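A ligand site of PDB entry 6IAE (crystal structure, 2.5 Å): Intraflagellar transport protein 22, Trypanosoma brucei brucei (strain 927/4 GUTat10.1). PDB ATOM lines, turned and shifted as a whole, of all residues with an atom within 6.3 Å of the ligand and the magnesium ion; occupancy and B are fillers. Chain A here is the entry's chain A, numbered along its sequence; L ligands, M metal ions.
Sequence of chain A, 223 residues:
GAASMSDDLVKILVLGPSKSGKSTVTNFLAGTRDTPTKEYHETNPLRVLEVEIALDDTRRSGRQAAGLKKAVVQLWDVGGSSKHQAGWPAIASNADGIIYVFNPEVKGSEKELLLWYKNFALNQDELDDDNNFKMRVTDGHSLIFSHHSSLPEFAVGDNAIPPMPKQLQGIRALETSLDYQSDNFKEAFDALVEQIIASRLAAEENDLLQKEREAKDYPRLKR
OG of Ser 20 lies within hydrogen-bond range of O2 of the ligand (3.4 Å).
O6 of the ligand sits at hydrogen-bond distance from OG1 of Thr 24 (3.2 Å).
N of Gly 21 sits at hydrogen-bond distance from O4 of the ligand.
The backbone NH (N) of Lys 19 lies within hydrogen-bond range of an oxygen (O2) of the ligand (2.7 Å).
O11 of the ligand lies close to N of Leu 178 (3.5 Å).
O3 of the ligand sits at hydrogen-bond distance from N of Lys 22, 2.8 Å away.
OD2 of Asp 179 sits at hydrogen-bond distance from N4 of the ligand (2.7 Å).
A ring nitrogen (NE2) of His 147 sits at hydrogen-bond distance from a nitrogen (N2) of the ligand (2.9 Å).
The backbone NH (N) of Ser 20 lies within hydrogen-bond range of an oxygen (O2) of the ligand, at 2.9 Å.
N4 of the ligand sits close to O of Ser 149, 3.1 Å away.
The backbone NH of Thr 24 is in hydrogen-bond range of an oxygen (O6) of the ligand (3.3 Å).
O of His 148 sits close to N3 of the ligand, 3.3 Å away.
The side-chain hydroxyl of Thr 43 lies close to an oxygen (O1) of the ligand.
OD1 of Asp 179 is in hydrogen-bond range of OG of Ser 177, at 2.7 Å.
The side-chain hydroxyl (OG) of Ser 149 lies within hydrogen-bond range of the backbone carbonyl oxygen (O) of Ser 20, 3.3 Å away.
The side-chain hydroxyl of Ser 177 is in hydrogen-bond range of the backbone NH of Tyr 180, 2.7 Å away.
O of Thr 176 is in hydrogen-bond range of N of His 148, at 2.6 Å.
The side-chain amino group (NZ) of Lys 22 lies within hydrogen-bond range of the backbone carbonyl oxygen (O) of Gly 16 (2.6 Å).
O of Asp 77 is in hydrogen-bond range of N of Arg 47.
The side-chain hydroxyl (OG) of Ser 177 lies within hydrogen-bond range of the backbone carbonyl oxygen (O) of His 148.
The side-chain amino group (NZ) of Lys 22 sits close to the backbone carbonyl oxygen (O) of Val 78 (3.4 Å).
The backbone carbonyl oxygen of Pro 17 sits close to an oxygen (O2) of the ligand (3.5 Å).
Residues that only touch the ligand: Ser 18 (3.3 Å) and Tyr 180 (3.9 Å).
Hydrophobic or aromatic side chains within 4 Å of the ligand: His 147, Leu 178 and Tyr 180.
Of the 26 residues printed, 15 come within 4 Å of the ligand.
Asn 44 touches the magnesium ion (OD1 to MG, 3.6 Å).
Asp 77 touches the magnesium ion (OD2 to MG, 3.9 Å).
The nearest printed residue that does not touch the magnesium ion is Glu 42 (5.1 Å).
The magnesium ion is bound by OG1 of Thr 43 (2.2 Å).
The magnesium ion has one donor atom within binding distance.
Slightly farther from the magnesium ion lies OG of Ser 23 (2.8 Å).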
ATOM      1  N   GLY A  16      32.025 -18.667 -20.183  1.00  0.00           N
ATOM      2  CA  GLY A  16      31.491 -19.947 -19.796  1.00  0.00           C
ATOM      3  C   GLY A  16      32.274 -21.083 -20.406  1.00  0.00           C
ATOM      4  O   GLY A  16      33.185 -20.864 -21.203  1.00  0.00           O
ATOM      5  N   PRO A  17      31.950 -22.326 -20.030  1.00  0.00           N
ATOM      6  CA  PRO A  17      32.643 -23.471 -20.623  1.00  0.00           C
ATOM      7  C   PRO A  17      32.618 -23.437 -22.142  1.00  0.00           C
ATOM      8  O   PRO A  17      31.701 -22.897 -22.764  1.00  0.00           O
ATOM      9  CB  PRO A  17      31.879 -24.673 -20.067  1.00  0.00           C
ATOM     10  CG  PRO A  17      31.382 -24.203 -18.755  1.00  0.00           C
ATOM     11  CD  PRO A  17      31.062 -22.743 -18.936  1.00  0.00           C
ATOM     12  N   SER A  18      33.666 -23.995 -22.744  1.00  0.00           N
ATOM     13  CA  SER A  18      33.664 -24.195 -24.172  1.00  0.00           C
ATOM     14  C   SER A  18      32.611 -25.226 -24.545  1.00  0.00           C
ATOM     15  O   SER A  18      32.162 -26.034 -23.719  1.00  0.00           O
ATOM     16  CB  SER A  18      35.045 -24.652 -24.629  1.00  0.00           C
ATOM     17  OG  SER A  18      35.635 -25.487 -23.641  1.00  0.00           O
ATOM     18  N   LYS A  19      32.186 -25.179 -25.815  1.00  0.00           N
ATOM     19  CA  LYS A  19      31.145 -26.050 -26.371  1.00  0.00           C
ATOM     20  C   LYS A  19      29.805 -25.874 -25.683  1.00  0.00           C
ATOM     21  O   LYS A  19      28.886 -26.683 -25.903  1.00  0.00           O
ATOM     22  CB  LYS A  19      31.568 -27.531 -26.340  1.00  0.00           C
ATOM     23  CG  LYS A  19      33.025 -27.785 -26.712  1.00  0.00           C
ATOM     24  CD  LYS A  19      33.582 -29.062 -26.067  1.00  0.00           C
ATOM     25  CE  LYS A  19      33.355 -29.083 -24.566  1.00  0.00           C
ATOM     26  NZ  LYS A  19      34.073 -30.204 -23.910  1.00  0.00           N
ATOM     27  N   SER A  20      29.659 -24.843 -24.846  1.00  0.00           N
ATOM     28  CA  SER A  20      28.444 -24.661 -24.068  1.00  0.00           C
ATOM     29  C   SER A  20      27.350 -24.018 -24.881  1.00  0.00           C
ATOM     30  O   SER A  20      26.174 -24.341 -24.691  1.00  0.00           O
ATOM     31  CB  SER A  20      28.747 -23.816 -22.830  1.00  0.00           C
ATOM     32  OG  SER A  20      29.435 -22.638 -23.204  1.00  0.00           O
ATOM     33  N   GLY A  21      27.703 -23.119 -25.792  1.00  0.00           N
ATOM     34  CA  GLY A  21      26.734 -22.499 -26.655  1.00  0.00           C
ATOM     35  C   GLY A  21      26.792 -20.991 -26.749  1.00  0.00           C
ATOM     36  O   GLY A  21      25.882 -20.387 -27.301  1.00  0.00           O
ATOM     37  N   LYS A  22      27.889 -20.373 -26.285  1.00  0.00           N
ATOM     38  CA  LYS A  22      27.865 -18.946 -25.997  1.00  0.00           C
ATOM     39  C   LYS A  22      27.502 -18.108 -27.216  1.00  0.00           C
ATOM     40  O   LYS A  22      26.841 -17.076 -27.077  1.00  0.00           O
ATOM     41  CB  LYS A  22      29.222 -18.468 -25.474  1.00  0.00           C
ATOM     42  CG  LYS A  22      29.986 -19.369 -24.505  1.00  0.00           C
ATOM     43  CD  LYS A  22      31.459 -19.271 -24.883  1.00  0.00           C
ATOM     44  CE  LYS A  22      32.392 -20.012 -23.934  1.00  0.00           C
ATOM     45  NZ  LYS A  22      33.103 -19.062 -23.054  1.00  0.00           N
ATOM     46  N   SER A  23      27.916 -18.514 -28.421  1.00  0.00           N
ATOM     47  CA  SER A  23      27.746 -17.675 -29.596  1.00  0.00           C
ATOM     48  C   SER A  23      26.414 -17.879 -30.296  1.00  0.00           C
ATOM     49  O   SER A  23      25.894 -16.937 -30.892  1.00  0.00           O
ATOM     50  CB  SER A  23      28.874 -17.922 -30.604  1.00  0.00           C
ATOM     51  OG  SER A  23      30.157 -17.906 -29.990  1.00  0.00           O
ATOM     52  N   THR A  24      25.836 -19.090 -30.234  1.00  0.00           N
ATOM     53  CA  THR A  24      24.462 -19.247 -30.705  1.00  0.00           C
ATOM     54  C   THR A  24      23.541 -18.281 -29.979  1.00  0.00           C
ATOM     55  O   THR A  24      22.553 -17.817 -30.563  1.00  0.00           O
ATOM     56  CB  THR A  24      23.989 -20.682 -30.505  1.00  0.00           C
ATOM     57  OG1 THR A  24      24.523 -21.205 -29.280  1.00  0.00           O
ATOM     58  CG2 THR A  24      24.423 -21.561 -31.686  1.00  0.00           C
ATOM     59  N   VAL A  25      23.867 -17.940 -28.731  1.00  0.00           N
ATOM     60  CA  VAL A  25      23.103 -16.941 -28.007  1.00  0.00           C
ATOM     61  C   VAL A  25      23.415 -15.543 -28.521  1.00  0.00           C
ATOM     62  O   VAL A  25      22.511 -14.733 -28.764  1.00  0.00           O
ATOM     63  CB  VAL A  25      23.371 -17.068 -26.491  1.00  0.00           C
ATOM     64  CG1 VAL A  25      22.781 -15.908 -25.763  1.00  0.00           C
ATOM     65  CG2 VAL A  25      22.788 -18.375 -25.965  1.00  0.00           C
ATOM     66  N   GLU A  42      36.449 -25.136 -33.513  1.00  0.00           N
ATOM     67  CA  GLU A  42      35.649 -24.315 -34.416  1.00  0.00           C
ATOM     68  C   GLU A  42      35.077 -23.094 -33.691  1.00  0.00           C
ATOM     69  O   GLU A  42      34.315 -22.313 -34.278  1.00  0.00           O
ATOM     70  CB  GLU A  42      34.538 -25.150 -35.045  1.00  0.00           C
ATOM     71  N   THR A  43      35.434 -22.938 -32.415  1.00  0.00           N
ATOM     72  CA  THR A  43      35.140 -21.701 -31.699  1.00  0.00           C
ATOM     73  C   THR A  43      36.335 -20.779 -31.810  1.00  0.00           C
ATOM     74  O   THR A  43      37.492 -21.211 -31.771  1.00  0.00           O
ATOM     75  CB  THR A  43      34.782 -21.981 -30.219  1.00  0.00           C
ATOM     76  OG1 THR A  43      33.943 -20.926 -29.731  1.00  0.00           O
ATOM     77  CG2 THR A  43      36.010 -22.085 -29.338  1.00  0.00           C
ATOM     78  N   ASN A  44      36.059 -19.534 -32.017  1.00  0.00           N
ATOM     79  CA  ASN A  44      36.999 -18.450 -32.256  1.00  0.00           C
ATOM     80  C   ASN A  44      37.364 -17.763 -30.947  1.00  0.00           C
ATOM     81  O   ASN A  44      36.583 -17.774 -29.996  1.00  0.00           O
ATOM     82  CB  ASN A  44      36.393 -17.436 -33.219  1.00  0.00           C
ATOM     83  CG  ASN A  44      34.902 -17.298 -33.041  1.00  0.00           C
ATOM     84  OD1 ASN A  44      34.382 -17.343 -31.919  1.00  0.00           O
ATOM     85  ND2 ASN A  44      34.187 -17.146 -34.142  1.00  0.00           N
ATOM     86  N   ARG A  47      34.620 -12.575 -30.661  1.00  0.00           N
ATOM     87  CA  ARG A  47      33.834 -11.781 -31.585  1.00  0.00           C
ATOM     88  C   ARG A  47      33.280 -10.601 -30.811  1.00  0.00           C
ATOM     89  O   ARG A  47      33.265 -10.600 -29.586  1.00  0.00           O
ATOM     90  CB  ARG A  47      32.693 -12.601 -32.197  1.00  0.00           C
ATOM     91  CG  ARG A  47      33.111 -13.399 -33.402  1.00  0.00           C
ATOM     92  CD  ARG A  47      32.012 -14.303 -33.900  1.00  0.00           C
ATOM     93  NE  ARG A  47      30.684 -13.824 -33.546  1.00  0.00           N
ATOM     94  CZ  ARG A  47      29.568 -14.508 -33.781  1.00  0.00           C
ATOM     95  NH1 ARG A  47      29.627 -15.697 -34.358  1.00  0.00           N
ATOM     96  NH2 ARG A  47      28.390 -14.002 -33.431  1.00  0.00           N
ATOM     97  N   ASP A  77      31.482 -12.016 -27.432  1.00  0.00           N
ATOM     98  CA  ASP A  77      31.567 -13.470 -27.306  1.00  0.00           C
ATOM     99  C   ASP A  77      33.017 -13.909 -27.185  1.00  0.00           C
ATOM    100  O   ASP A  77      33.809 -13.718 -28.122  1.00  0.00           O
ATOM    101  CB  ASP A  77      30.896 -14.148 -28.490  1.00  0.00           C
ATOM    102  CG  ASP A  77      31.359 -15.575 -28.686  1.00  0.00           C
ATOM    103  OD1 ASP A  77      31.373 -16.352 -27.708  1.00  0.00           O
ATOM    104  OD2 ASP A  77      31.737 -15.929 -29.819  1.00  0.00           O
ATOM    105  N   VAL A  78      33.366 -14.522 -26.062  1.00  0.00           N
ATOM    106  CA  VAL A  78      34.726 -14.944 -25.740  1.00  0.00           C
ATOM    107  C   VAL A  78      34.860 -16.443 -25.952  1.00  0.00           C
ATOM    108  O   VAL A  78      33.900 -17.198 -25.799  1.00  0.00           O
ATOM    109  CB  VAL A  78      35.075 -14.543 -24.292  1.00  0.00           C
ATOM    110  CG1 VAL A  78      36.458 -15.056 -23.897  1.00  0.00           C
ATOM    111  CG2 VAL A  78      34.977 -13.040 -24.121  1.00  0.00           C
ATOM    112  N   GLY A  79      36.064 -16.871 -26.328  1.00  0.00           N
ATOM    113  CA  GLY A  79      36.389 -18.295 -26.421  1.00  0.00           C
ATOM    114  C   GLY A  79      37.539 -18.639 -25.485  1.00  0.00           C
ATOM    115  O   GLY A  79      38.524 -17.893 -25.400  1.00  0.00           O
ATOM    116  N   HIS A 147      21.973 -24.149 -20.437  1.00  0.00           N
ATOM    117  CA  HIS A 147      21.668 -24.093 -21.866  1.00  0.00           C
ATOM    118  C   HIS A 147      21.605 -25.479 -22.482  1.00  0.00           C
ATOM    119  O   HIS A 147      22.591 -26.231 -22.436  1.00  0.00           O
ATOM    120  CB  HIS A 147      22.692 -23.238 -22.603  1.00  0.00           C
ATOM    121  CG  HIS A 147      22.455 -23.164 -24.082  1.00  0.00           C
ATOM    122  ND1 HIS A 147      21.640 -22.219 -24.659  1.00  0.00           N
ATOM    123  CD2 HIS A 147      22.910 -23.935 -25.096  1.00  0.00           C
ATOM    124  CE1 HIS A 147      21.609 -22.400 -25.958  1.00  0.00           C
ATOM    125  NE2 HIS A 147      22.375 -23.441 -26.248  1.00  0.00           N
ATOM    126  N   HIS A 148      20.469 -25.795 -23.114  1.00  0.00           N
ATOM    127  CA  HIS A 148      20.255 -27.063 -23.790  1.00  0.00           C
ATOM    128  C   HIS A 148      20.707 -26.950 -25.238  1.00  0.00           C
ATOM    129  O   HIS A 148      20.024 -26.318 -26.049  1.00  0.00           O
ATOM    130  CB  HIS A 148      18.790 -27.485 -23.724  1.00  0.00           C
ATOM    131  CG  HIS A 148      18.335 -27.881 -22.356  1.00  0.00           C
ATOM    132  ND1 HIS A 148      17.016 -27.843 -21.978  1.00  0.00           N
ATOM    133  CD2 HIS A 148      19.028 -28.329 -21.285  1.00  0.00           C
ATOM    134  CE1 HIS A 148      16.912 -28.242 -20.726  1.00  0.00           C
ATOM    135  NE2 HIS A 148      18.116 -28.546 -20.276  1.00  0.00           N
ATOM    136  N   SER A 149      21.850 -27.562 -25.550  1.00  0.00           N
ATOM    137  CA  SER A 149      22.276 -27.850 -26.920  1.00  0.00           C
ATOM    138  C   SER A 149      21.893 -29.253 -27.345  1.00  0.00           C
ATOM    139  O   SER A 149      22.085 -29.603 -28.519  1.00  0.00           O
ATOM    140  CB  SER A 149      23.798 -27.698 -27.040  1.00  0.00           C
ATOM    141  OG  SER A 149      24.287 -26.632 -26.241  1.00  0.00           O
ATOM    142  N   SER A 150      21.388 -30.062 -26.421  1.00  0.00           N
ATOM    143  CA  SER A 150      21.121 -31.487 -26.620  1.00  0.00           C
ATOM    144  C   SER A 150      19.780 -31.818 -26.000  1.00  0.00           C
ATOM    145  O   SER A 150      19.153 -30.985 -25.347  1.00  0.00           O
ATOM    146  CB  SER A 150      22.198 -32.361 -25.971  1.00  0.00           C
ATOM    147  OG  SER A 150      21.821 -32.735 -24.660  1.00  0.00           O
ATOM    148  N   THR A 176      17.632 -22.694 -20.788  1.00  0.00           N
ATOM    149  CA  THR A 176      17.732 -21.999 -22.056  1.00  0.00           C
ATOM    150  C   THR A 176      17.929 -22.965 -23.217  1.00  0.00           C
ATOM    151  O   THR A 176      18.686 -23.934 -23.111  1.00  0.00           O
ATOM    152  CB  THR A 176      18.880 -20.978 -22.007  1.00  0.00           C
ATOM    153  OG1 THR A 176      18.429 -19.826 -21.291  1.00  0.00           O
ATOM    154  CG2 THR A 176      19.310 -20.579 -23.387  1.00  0.00           C
ATOM    155  N   SER A 177      17.228 -22.700 -24.311  1.00  0.00           N
ATOM    156  CA  SER A 177      17.376 -23.460 -25.536  1.00  0.00           C
ATOM    157  C   SER A 177      16.658 -22.714 -26.644  1.00  0.00           C
ATOM    158  O   SER A 177      15.783 -21.872 -26.388  1.00  0.00           O
ATOM    159  CB  SER A 177      16.809 -24.868 -25.396  1.00  0.00           C
ATOM    160  OG  SER A 177      16.779 -25.487 -26.653  1.00  0.00           O
ATOM    161  N   LEU A 178      17.037 -23.014 -27.876  1.00  0.00           N
ATOM    162  CA  LEU A 178      16.308 -22.502 -29.032  1.00  0.00           C
ATOM    163  C   LEU A 178      15.218 -23.453 -29.483  1.00  0.00           C
ATOM    164  O   LEU A 178      14.188 -23.010 -30.003  1.00  0.00           O
ATOM    165  CB  LEU A 178      17.263 -22.244 -30.197  1.00  0.00           C
ATOM    166  CG  LEU A 178      18.124 -20.983 -30.205  1.00  0.00           C
ATOM    167  CD1 LEU A 178      19.347 -21.157 -29.302  1.00  0.00           C
ATOM    168  CD2 LEU A 178      18.538 -20.635 -31.617  1.00  0.00           C
ATOM    169  N   ASP A 179      15.421 -24.756 -29.275  1.00  0.00           N
ATOM    170  CA  ASP A 179      14.487 -25.787 -29.694  1.00  0.00           C
ATOM    171  C   ASP A 179      13.878 -26.542 -28.527  1.00  0.00           C
ATOM    172  O   ASP A 179      12.679 -26.838 -28.542  1.00  0.00           O
ATOM    173  CB  ASP A 179      15.210 -26.769 -30.620  1.00  0.00           C
ATOM    174  CG  ASP A 179      16.646 -26.981 -30.226  1.00  0.00           C
ATOM    175  OD1 ASP A 179      17.013 -26.518 -29.118  1.00  0.00           O
ATOM    176  OD2 ASP A 179      17.407 -27.601 -31.005  1.00  0.00           O
ATOM    177  N   TYR A 180      14.678 -26.866 -27.521  1.00  0.00           N
ATOM    178  CA  TYR A 180      14.189 -27.633 -26.375  1.00  0.00           C
ATOM    179  C   TYR A 180      13.448 -26.682 -25.440  1.00  0.00           C
ATOM    180  O   TYR A 180      13.131 -25.545 -25.790  1.00  0.00           O
ATOM    181  CB  TYR A 180      15.362 -28.367 -25.719  1.00  0.00           C
ATOM    182  CG  TYR A 180      15.921 -29.510 -26.555  1.00  0.00           C
ATOM    183  CD1 TYR A 180      15.248 -30.708 -26.685  1.00  0.00           C
ATOM    184  CD2 TYR A 180      17.128 -29.368 -27.234  1.00  0.00           C
ATOM    185  CE1 TYR A 180      15.741 -31.743 -27.450  1.00  0.00           C
ATOM    186  CE2 TYR A 180      17.641 -30.408 -28.010  1.00  0.00           C
ATOM    187  CZ  TYR A 180      16.939 -31.597 -28.110  1.00  0.00           C
ATOM    188  OH  TYR A 180      17.409 -32.656 -28.869  1.00  0.00           O
HETATM  189  O1  LIG L   1      31.906 -22.508 -28.614  1.00  0.00           O
HETATM  190  P1  LIG L   1      30.757 -22.199 -27.528  1.00  0.00           P
HETATM  191  O2  LIG L   1      31.145 -22.761 -26.195  1.00  0.00           O
HETATM  192  O3  LIG L   1      30.452 -20.729 -27.446  1.00  0.00           O
HETATM  193  O4  LIG L   1      29.425 -22.901 -28.073  1.00  0.00           O
HETATM  194  P2  LIG L   1      28.905 -22.572 -29.532  1.00  0.00           P
HETATM  195  O5  LIG L   1      29.933 -21.813 -30.337  1.00  0.00           O
HETATM  196  O6  LIG L   1      27.601 -21.831 -29.533  1.00  0.00           O
HETATM  197  O7  LIG L   1      28.649 -24.040 -30.121  1.00  0.00           O
HETATM  198  C1  LIG L   1      27.574 -24.786 -29.620  1.00  0.00           C
HETATM  199  C2  LIG L   1      27.145 -25.790 -30.683  1.00  0.00           C
HETATM  200  O8  LIG L   1      26.170 -26.628 -30.106  1.00  0.00           O
HETATM  201  C3  LIG L   1      26.507 -25.082 -31.869  1.00  0.00           C
HETATM  202  O9  LIG L   1      27.320 -25.099 -33.023  1.00  0.00           O
HETATM  203  C4  LIG L   1      25.229 -25.841 -32.154  1.00  0.00           C
HETATM  204  O10 LIG L   1      25.365 -26.675 -33.280  1.00  0.00           O
HETATM  205  C5  LIG L   1      24.989 -26.614 -30.869  1.00  0.00           C
HETATM  206  N1  LIG L   1      24.022 -25.813 -30.132  1.00  0.00           N
HETATM  207  C6  LIG L   1      24.233 -24.601 -29.513  1.00  0.00           C
HETATM  208  N2  LIG L   1      23.078 -24.187 -28.966  1.00  0.00           N
HETATM  209  C7  LIG L   1      22.132 -25.112 -29.232  1.00  0.00           C
HETATM  210  C8  LIG L   1      20.783 -25.198 -28.910  1.00  0.00           C
HETATM  211  O11 LIG L   1      20.252 -24.289 -28.250  1.00  0.00           O
HETATM  212  N3  LIG L   1      20.051 -26.290 -29.323  1.00  0.00           N
HETATM  213  C9  LIG L   1      20.653 -27.309 -30.063  1.00  0.00           C
HETATM  214  N4  LIG L   1      19.951 -28.361 -30.459  1.00  0.00           N
HETATM  215  N5  LIG L   1      21.989 -27.211 -30.371  1.00  0.00           N
HETATM  216  C10 LIG L   1      22.709 -26.133 -29.971  1.00  0.00           C
HETATM  217 MG    MG M   1      32.214 -19.735 -30.410  1.00  0.00          MG
